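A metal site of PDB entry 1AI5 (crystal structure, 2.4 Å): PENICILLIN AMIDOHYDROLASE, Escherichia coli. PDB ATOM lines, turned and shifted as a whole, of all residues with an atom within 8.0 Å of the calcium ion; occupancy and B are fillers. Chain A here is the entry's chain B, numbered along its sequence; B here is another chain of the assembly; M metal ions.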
ATOM      1  N   GLY A  72      10.909   3.835 -19.582  1.00  0.00           N
ATOM      2  CA  GLY A  72      11.445   4.632 -20.703  1.00  0.00           C
ATOM      3  C   GLY A  72      10.264   5.514 -21.105  1.00  0.00           C
ATOM      4  O   GLY A  72       9.147   5.268 -20.634  1.00  0.00           O
ATOM      5  N   ASP A  73      10.510   6.490 -21.964  1.00  0.00           N
ATOM      6  CA  ASP A  73       9.405   7.346 -22.410  1.00  0.00           C
ATOM      7  C   ASP A  73       8.782   6.722 -23.667  1.00  0.00           C
ATOM      8  O   ASP A  73       9.247   6.828 -24.809  1.00  0.00           O
ATOM      9  CB  ASP A  73       9.870   8.797 -22.618  1.00  0.00           C
ATOM     10  CG  ASP A  73       8.776   9.715 -23.070  1.00  0.00           C
ATOM     11  OD1 ASP A  73       7.728   9.191 -23.513  1.00  0.00           O
ATOM     12  OD2 ASP A  73       8.702  10.970 -23.069  1.00  0.00           O
ATOM     13  N   ASP A  74       7.564   6.177 -23.520  1.00  0.00           N
ATOM     14  CA  ASP A  74       6.972   5.524 -24.670  1.00  0.00           C
ATOM     15  C   ASP A  74       5.596   6.059 -24.934  1.00  0.00           C
ATOM     16  O   ASP A  74       4.780   5.408 -25.579  1.00  0.00           O
ATOM     17  CB  ASP A  74       6.977   4.000 -24.525  1.00  0.00           C
ATOM     18  CG  ASP A  74       6.262   3.521 -23.283  1.00  0.00           C
ATOM     19  OD1 ASP A  74       5.713   4.291 -22.486  1.00  0.00           O
ATOM     20  OD2 ASP A  74       6.230   2.328 -22.983  1.00  0.00           O
ATOM     21  N   VAL A  75       5.273   7.130 -24.225  1.00  0.00           N
ATOM     22  CA  VAL A  75       3.996   7.793 -24.364  1.00  0.00           C
ATOM     23  C   VAL A  75       4.215   9.302 -24.575  1.00  0.00           C
ATOM     24  O   VAL A  75       4.801   9.924 -23.682  1.00  0.00           O
ATOM     25  CB  VAL A  75       3.203   7.584 -23.061  1.00  0.00           C
ATOM     26  CG1 VAL A  75       1.881   8.348 -23.119  1.00  0.00           C
ATOM     27  CG2 VAL A  75       2.847   6.128 -22.836  1.00  0.00           C
ATOM     28  N   ASP A  76       3.562   9.905 -25.574  1.00  0.00           N
ATOM     29  CA  ASP A  76       3.656  11.354 -25.763  1.00  0.00           C
ATOM     30  C   ASP A  76       2.200  11.827 -25.955  1.00  0.00           C
ATOM     31  O   ASP A  76       1.373  11.027 -26.420  1.00  0.00           O
ATOM     32  CB  ASP A  76       4.470  11.822 -26.968  1.00  0.00           C
ATOM     33  CG  ASP A  76       5.914  11.473 -26.964  1.00  0.00           C
ATOM     34  OD1 ASP A  76       6.584  11.308 -25.897  1.00  0.00           O
ATOM     35  OD2 ASP A  76       6.531  11.346 -28.061  1.00  0.00           O
ATOM     36  N   ILE A  77       1.954  13.093 -25.702  1.00  0.00           N
ATOM     37  CA  ILE A  77       0.600  13.627 -25.788  1.00  0.00           C
ATOM     38  C   ILE A  77       0.525  14.525 -27.030  1.00  0.00           C
ATOM     39  O   ILE A  77       1.432  15.327 -27.262  1.00  0.00           O
ATOM     40  CB  ILE A  77       0.324  14.487 -24.544  1.00  0.00           C
ATOM     41  CG1 ILE A  77       0.388  13.713 -23.229  1.00  0.00           C
ATOM     42  CG2 ILE A  77      -0.950  15.307 -24.610  1.00  0.00           C
ATOM     43  CD1 ILE A  77      -0.652  12.655 -23.043  1.00  0.00           C
ATOM     44  N   SER A 140      -0.782   9.178 -26.859  1.00  0.00           N
ATOM     45  CA  SER A 140      -0.339   8.247 -27.860  1.00  0.00           C
ATOM     46  C   SER A 140       0.776   7.327 -27.382  1.00  0.00           C
ATOM     47  O   SER A 140       1.802   7.761 -26.920  1.00  0.00           O
ATOM     48  CB  SER A 140      -0.051   9.040 -29.126  1.00  0.00           C
ATOM     49  OG  SER A 140       0.973   8.383 -29.844  1.00  0.00           O
ATOM     50  N   PRO A 197       9.184   5.417 -29.885  1.00  0.00           N
ATOM     51  CA  PRO A 197       8.876   6.207 -31.052  1.00  0.00           C
ATOM     52  C   PRO A 197      10.063   6.783 -31.790  1.00  0.00           C
ATOM     53  O   PRO A 197      11.087   6.997 -31.176  1.00  0.00           O
ATOM     54  CB  PRO A 197       7.915   7.336 -30.612  1.00  0.00           C
ATOM     55  CG  PRO A 197       8.147   7.377 -29.127  1.00  0.00           C
ATOM     56  CD  PRO A 197       8.724   6.076 -28.658  1.00  0.00           C
ATOM     57  N   ARG A 199      11.134   9.939 -33.181  1.00  0.00           N
ATOM     58  CA  ARG A 199      10.556  11.262 -33.159  1.00  0.00           C
ATOM     59  C   ARG A 199      11.204  12.191 -34.184  1.00  0.00           C
ATOM     60  O   ARG A 199      12.367  12.035 -34.505  1.00  0.00           O
ATOM     61  CB  ARG A 199      10.635  11.836 -31.727  1.00  0.00           C
ATOM     62  CG  ARG A 199       9.792  11.075 -30.700  1.00  0.00           C
ATOM     63  CD  ARG A 199      10.155  11.537 -29.289  1.00  0.00           C
ATOM     64  NE  ARG A 199       9.192  11.085 -28.269  1.00  0.00           N
ATOM     65  CZ  ARG A 199       9.622  10.109 -27.438  1.00  0.00           C
ATOM     66  NH1 ARG A 199      10.827   9.587 -27.514  1.00  0.00           N
ATOM     67  NH2 ARG A 199       8.769   9.713 -26.520  1.00  0.00           N
ATOM     68  N   HIS A 203      11.548  17.606 -31.467  1.00  0.00           N
ATOM     69  CA  HIS A 203      10.540  17.098 -30.556  1.00  0.00           C
ATOM     70  C   HIS A 203      11.125  16.990 -29.139  1.00  0.00           C
ATOM     71  O   HIS A 203      12.038  16.218 -28.918  1.00  0.00           O
ATOM     72  CB  HIS A 203      10.134  15.692 -31.067  1.00  0.00           C
ATOM     73  CG  HIS A 203       8.961  15.179 -30.299  1.00  0.00           C
ATOM     74  ND1 HIS A 203       7.933  14.430 -30.846  1.00  0.00           N
ATOM     75  CD2 HIS A 203       8.627  15.301 -28.988  1.00  0.00           C
ATOM     76  CE1 HIS A 203       7.029  14.128 -29.943  1.00  0.00           C
ATOM     77  NE2 HIS A 203       7.456  14.650 -28.791  1.00  0.00           N
ATOM     78  N   ASP A 204      10.687  17.760 -28.159  1.00  0.00           N
ATOM     79  CA  ASP A 204      11.146  17.610 -26.771  1.00  0.00           C
ATOM     80  C   ASP A 204      10.103  16.663 -26.151  1.00  0.00           C
ATOM     81  O   ASP A 204       8.931  17.020 -26.080  1.00  0.00           O
ATOM     82  CB  ASP A 204      11.156  18.962 -26.080  1.00  0.00           C
ATOM     83  CG  ASP A 204      11.540  18.942 -24.611  1.00  0.00           C
ATOM     84  OD1 ASP A 204      11.436  17.878 -23.933  1.00  0.00           O
ATOM     85  OD2 ASP A 204      11.995  20.007 -24.139  1.00  0.00           O
ATOM     86  N   PRO A 205      10.467  15.452 -25.803  1.00  0.00           N
ATOM     87  CA  PRO A 205       9.538  14.429 -25.383  1.00  0.00           C
ATOM     88  C   PRO A 205       8.970  14.649 -24.007  1.00  0.00           C
ATOM     89  O   PRO A 205       8.072  13.912 -23.584  1.00  0.00           O
ATOM     90  CB  PRO A 205      10.268  13.072 -25.544  1.00  0.00           C
ATOM     91  CG  PRO A 205      11.696  13.540 -25.373  1.00  0.00           C
ATOM     92  CD  PRO A 205      11.842  14.951 -25.902  1.00  0.00           C
ATOM     93  N   ARG A 206       9.318  15.752 -23.287  1.00  0.00           N
ATOM     94  CA  ARG A 206       8.777  15.990 -21.969  1.00  0.00           C
ATOM     95  C   ARG A 206       7.515  16.802 -21.990  1.00  0.00           C
ATOM     96  O   ARG A 206       6.952  16.969 -20.882  1.00  0.00           O
ATOM     97  CB  ARG A 206       9.750  16.719 -21.025  1.00  0.00           C
ATOM     98  CG  ARG A 206      11.097  15.967 -20.931  1.00  0.00           C
ATOM     99  CD  ARG A 206      12.208  16.894 -20.492  1.00  0.00           C
ATOM    100  NE  ARG A 206      12.445  18.056 -21.314  1.00  0.00           N
ATOM    101  CZ  ARG A 206      13.364  19.021 -21.078  1.00  0.00           C
ATOM    102  NH1 ARG A 206      14.166  18.884 -20.034  1.00  0.00           N
ATOM    103  NH2 ARG A 206      13.494  20.057 -21.900  1.00  0.00           N
ATOM    104  N   LEU A 207       7.156  17.317 -23.151  1.00  0.00           N
ATOM    105  CA  LEU A 207       5.995  18.222 -23.252  1.00  0.00           C
ATOM    106  C   LEU A 207       5.171  17.886 -24.489  1.00  0.00           C
ATOM    107  O   LEU A 207       5.690  17.353 -25.472  1.00  0.00           O
ATOM    108  CB  LEU A 207       6.515  19.673 -23.368  1.00  0.00           C
ATOM    109  CG  LEU A 207       7.527  20.183 -22.329  1.00  0.00           C
ATOM    110  CD1 LEU A 207       8.570  21.123 -22.901  1.00  0.00           C
ATOM    111  CD2 LEU A 207       6.765  20.830 -21.183  1.00  0.00           C
ATOM    112  N   PRO A 208       3.961  18.347 -24.592  1.00  0.00           N
ATOM    113  CA  PRO A 208       3.049  18.034 -25.674  1.00  0.00           C
ATOM    114  C   PRO A 208       3.464  18.532 -27.037  1.00  0.00           C
ATOM    115  O   PRO A 208       4.320  19.401 -27.160  1.00  0.00           O
ATOM    116  CB  PRO A 208       1.671  18.644 -25.294  1.00  0.00           C
ATOM    117  CG  PRO A 208       1.810  18.831 -23.813  1.00  0.00           C
ATOM    118  CD  PRO A 208       3.266  18.959 -23.446  1.00  0.00           C
ATOM    119  N   TRP A 217       5.075  11.070 -35.134  1.00  0.00           N
ATOM    120  CA  TRP A 217       6.219  10.178 -35.094  1.00  0.00           C
ATOM    121  C   TRP A 217       6.455   9.689 -36.525  1.00  0.00           C
ATOM    122  O   TRP A 217       5.574   9.678 -37.394  1.00  0.00           O
ATOM    123  CB  TRP A 217       5.899   8.973 -34.206  1.00  0.00           C
ATOM    124  CG  TRP A 217       5.618   9.261 -32.769  1.00  0.00           C
ATOM    125  CD1 TRP A 217       6.035  10.352 -32.042  1.00  0.00           C
ATOM    126  CD2 TRP A 217       4.976   8.387 -31.847  1.00  0.00           C
ATOM    127  NE1 TRP A 217       5.636  10.212 -30.747  1.00  0.00           N
ATOM    128  CE2 TRP A 217       5.000   9.015 -30.577  1.00  0.00           C
ATOM    129  CE3 TRP A 217       4.361   7.131 -31.971  1.00  0.00           C
ATOM    130  CZ2 TRP A 217       4.440   8.437 -29.447  1.00  0.00           C
ATOM    131  CZ3 TRP A 217       3.780   6.573 -30.834  1.00  0.00           C
ATOM    132  CH2 TRP A 217       3.840   7.207 -29.591  1.00  0.00           C
ATOM    133  N   ALA A 250      14.629   9.013 -19.538  1.00  0.00           N
ATOM    134  CA  ALA A 250      13.617   8.371 -18.730  1.00  0.00           C
ATOM    135  C   ALA A 250      12.228   8.855 -19.097  1.00  0.00           C
ATOM    136  O   ALA A 250      12.013   9.868 -19.762  1.00  0.00           O
ATOM    137  CB  ALA A 250      13.901   8.845 -17.286  1.00  0.00           C
ATOM    138  N   SER A 251      11.263   8.186 -18.515  1.00  0.00           N
ATOM    139  CA  SER A 251       9.839   8.578 -18.599  1.00  0.00           C
ATOM    140  C   SER A 251       9.779  10.102 -18.424  1.00  0.00           C
ATOM    141  O   SER A 251      10.539  10.644 -17.623  1.00  0.00           O
ATOM    142  CB  SER A 251       9.184   7.967 -17.364  1.00  0.00           C
ATOM    143  OG  SER A 251       7.826   8.331 -17.274  1.00  0.00           O
ATOM    144  N   ASP A 252       8.821  10.763 -18.988  1.00  0.00           N
ATOM    145  CA  ASP A 252       8.567  12.178 -18.832  1.00  0.00           C
ATOM    146  C   ASP A 252       7.871  12.553 -17.529  1.00  0.00           C
ATOM    147  O   ASP A 252       7.678  13.764 -17.304  1.00  0.00           O
ATOM    148  CB  ASP A 252       7.802  12.749 -20.020  1.00  0.00           C
ATOM    149  CG  ASP A 252       6.397  12.232 -20.189  1.00  0.00           C
ATOM    150  OD1 ASP A 252       5.589  12.180 -19.213  1.00  0.00           O
ATOM    151  OD2 ASP A 252       6.082  11.890 -21.374  1.00  0.00           O
ATOM    152  N   LEU A 253       7.516  11.617 -16.637  1.00  0.00           N
ATOM    153  CA  LEU A 253       6.923  11.963 -15.361  1.00  0.00           C
ATOM    154  C   LEU A 253       7.763  13.004 -14.598  1.00  0.00           C
ATOM    155  O   LEU A 253       8.916  12.700 -14.244  1.00  0.00           O
ATOM    156  CB  LEU A 253       6.870  10.742 -14.443  1.00  0.00           C
ATOM    157  CG  LEU A 253       5.843   9.689 -14.805  1.00  0.00           C
ATOM    158  CD1 LEU A 253       6.106   8.438 -13.965  1.00  0.00           C
ATOM    159  CD2 LEU A 253       4.417  10.214 -14.600  1.00  0.00           C
ATOM    160  N   SER B 149       2.826   5.614 -18.346  1.00  0.00           N
ATOM    161  CA  SER B 149       3.116   6.808 -17.539  1.00  0.00           C
ATOM    162  C   SER B 149       3.420   8.078 -18.297  1.00  0.00           C
ATOM    163  O   SER B 149       4.445   8.016 -19.015  1.00  0.00           O
ATOM    164  CB  SER B 149       4.385   6.437 -16.760  1.00  0.00           C
ATOM    165  OG  SER B 149       4.080   5.574 -15.736  1.00  0.00           O
ATOM    166  N   THR B 150       2.723   9.168 -18.094  1.00  0.00           N
ATOM    167  CA  THR B 150       3.128  10.427 -18.709  1.00  0.00           C
ATOM    168  C   THR B 150       2.627  11.538 -17.793  1.00  0.00           C
ATOM    169  O   THR B 150       1.598  11.332 -17.137  1.00  0.00           O
ATOM    170  CB  THR B 150       2.630  10.577 -20.155  1.00  0.00           C
ATOM    171  OG1 THR B 150       3.071  11.786 -20.772  1.00  0.00           O
ATOM    172  CG2 THR B 150       1.105  10.638 -20.155  1.00  0.00           C
ATOM    173  N   SER B 151       3.205  12.725 -17.830  1.00  0.00           N
ATOM    174  CA  SER B 151       2.728  13.870 -17.061  1.00  0.00           C
ATOM    175  C   SER B 151       2.962  15.111 -17.937  1.00  0.00           C
ATOM    176  O   SER B 151       2.861  16.207 -17.373  1.00  0.00           O
ATOM    177  CB  SER B 151       3.373  14.066 -15.663  1.00  0.00           C
ATOM    178  OG  SER B 151       4.797  14.239 -15.760  1.00  0.00           O
ATOM    179  N   GLU B 152       2.905  14.913 -19.261  1.00  0.00           N
ATOM    180  CA  GLU B 152       3.283  15.938 -20.218  1.00  0.00           C
ATOM    181  C   GLU B 152       2.459  17.211 -20.058  1.00  0.00           C
ATOM    182  O   GLU B 152       2.977  18.350 -20.132  1.00  0.00           O
ATOM    183  CB  GLU B 152       3.335  15.486 -21.670  1.00  0.00           C
ATOM    184  CG  GLU B 152       4.566  14.715 -22.089  1.00  0.00           C
ATOM    185  CD  GLU B 152       4.509  14.232 -23.540  1.00  0.00           C
ATOM    186  OE1 GLU B 152       3.711  14.846 -24.296  1.00  0.00           O
ATOM    187  OE2 GLU B 152       5.241  13.278 -23.941  1.00  0.00           O
ATOM    188  N   ASN B 155       3.687  18.892 -16.883  1.00  0.00           N
ATOM    189  CA  ASN B 155       4.974  19.486 -17.140  1.00  0.00           C
ATOM    190  C   ASN B 155       4.801  20.860 -17.836  1.00  0.00           C
ATOM    191  O   ASN B 155       5.525  21.808 -17.511  1.00  0.00           O
ATOM    192  CB  ASN B 155       5.836  18.575 -17.958  1.00  0.00           C
ATOM    193  CG  ASN B 155       6.160  17.242 -17.324  1.00  0.00           C
ATOM    194  OD1 ASN B 155       6.729  16.394 -18.033  1.00  0.00           O
ATOM    195  ND2 ASN B 155       5.776  17.025 -16.086  1.00  0.00           N
HETATM  196 CA    CA M   1       6.697  11.724 -23.584  1.00  0.00          CA
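OE2 of Glu 152 of chain B binds the calcium ion, 2.2 Å away.
The calcium ion is bound by the side-chain carboxylate (OD2) of Asp 73 (2.2 Å).
OD2 of Asp 252 is bound to the calcium ion (2.3 Å).
The calcium ion is bound by the side-chain carboxylate (OD1) of Asp 76 (2.4 Å).
O of Pro 205 is bound to the calcium ion.
The calcium ion is bound by O of Val 75 (2.6 Å).
The side-chain carboxylate (OD1) of Asp 73 is bound to the calcium ion (2.7 Å).
OG1 of Thr 150 of chain B lies within hydrogen-bond range of OD1 of Asp 252 (3.0 Å).
The backbone carbonyl oxygen of Asp 76 sits at hydrogen-bond distance from the backbone NH of Ser 140, 2.9 Å away.
The backbone carbonyl oxygen (O) of Asp 73 lies within hydrogen-bond range of the guanidinium group (NH2) of Arg 199 (3.4 Å).
O of Asp 252 sits close to OD1 of Asn 155 of chain B.
OE1 of Glu 152 of chain B sits at hydrogen-bond distance from N of Ile 77 (2.9 Å).
The side-chain carboxylate of Asp 76 is in salt-bridge range of the guanidinium group of Arg 199, 2.7 Å away.
OG1 of Thr 150 of chain B sits at hydrogen-bond distance from N of Glu 152 of chain B (3.5 Å).
The side-chain carboxylate (OD2) of Asp 76 lies within hydrogen-bond range of the indole nitrogen (NE1) of Trp 217, at 3.0 Å.
The nearest printed residue that does not touch the calcium ion is Arg 199 (4.1 Å).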
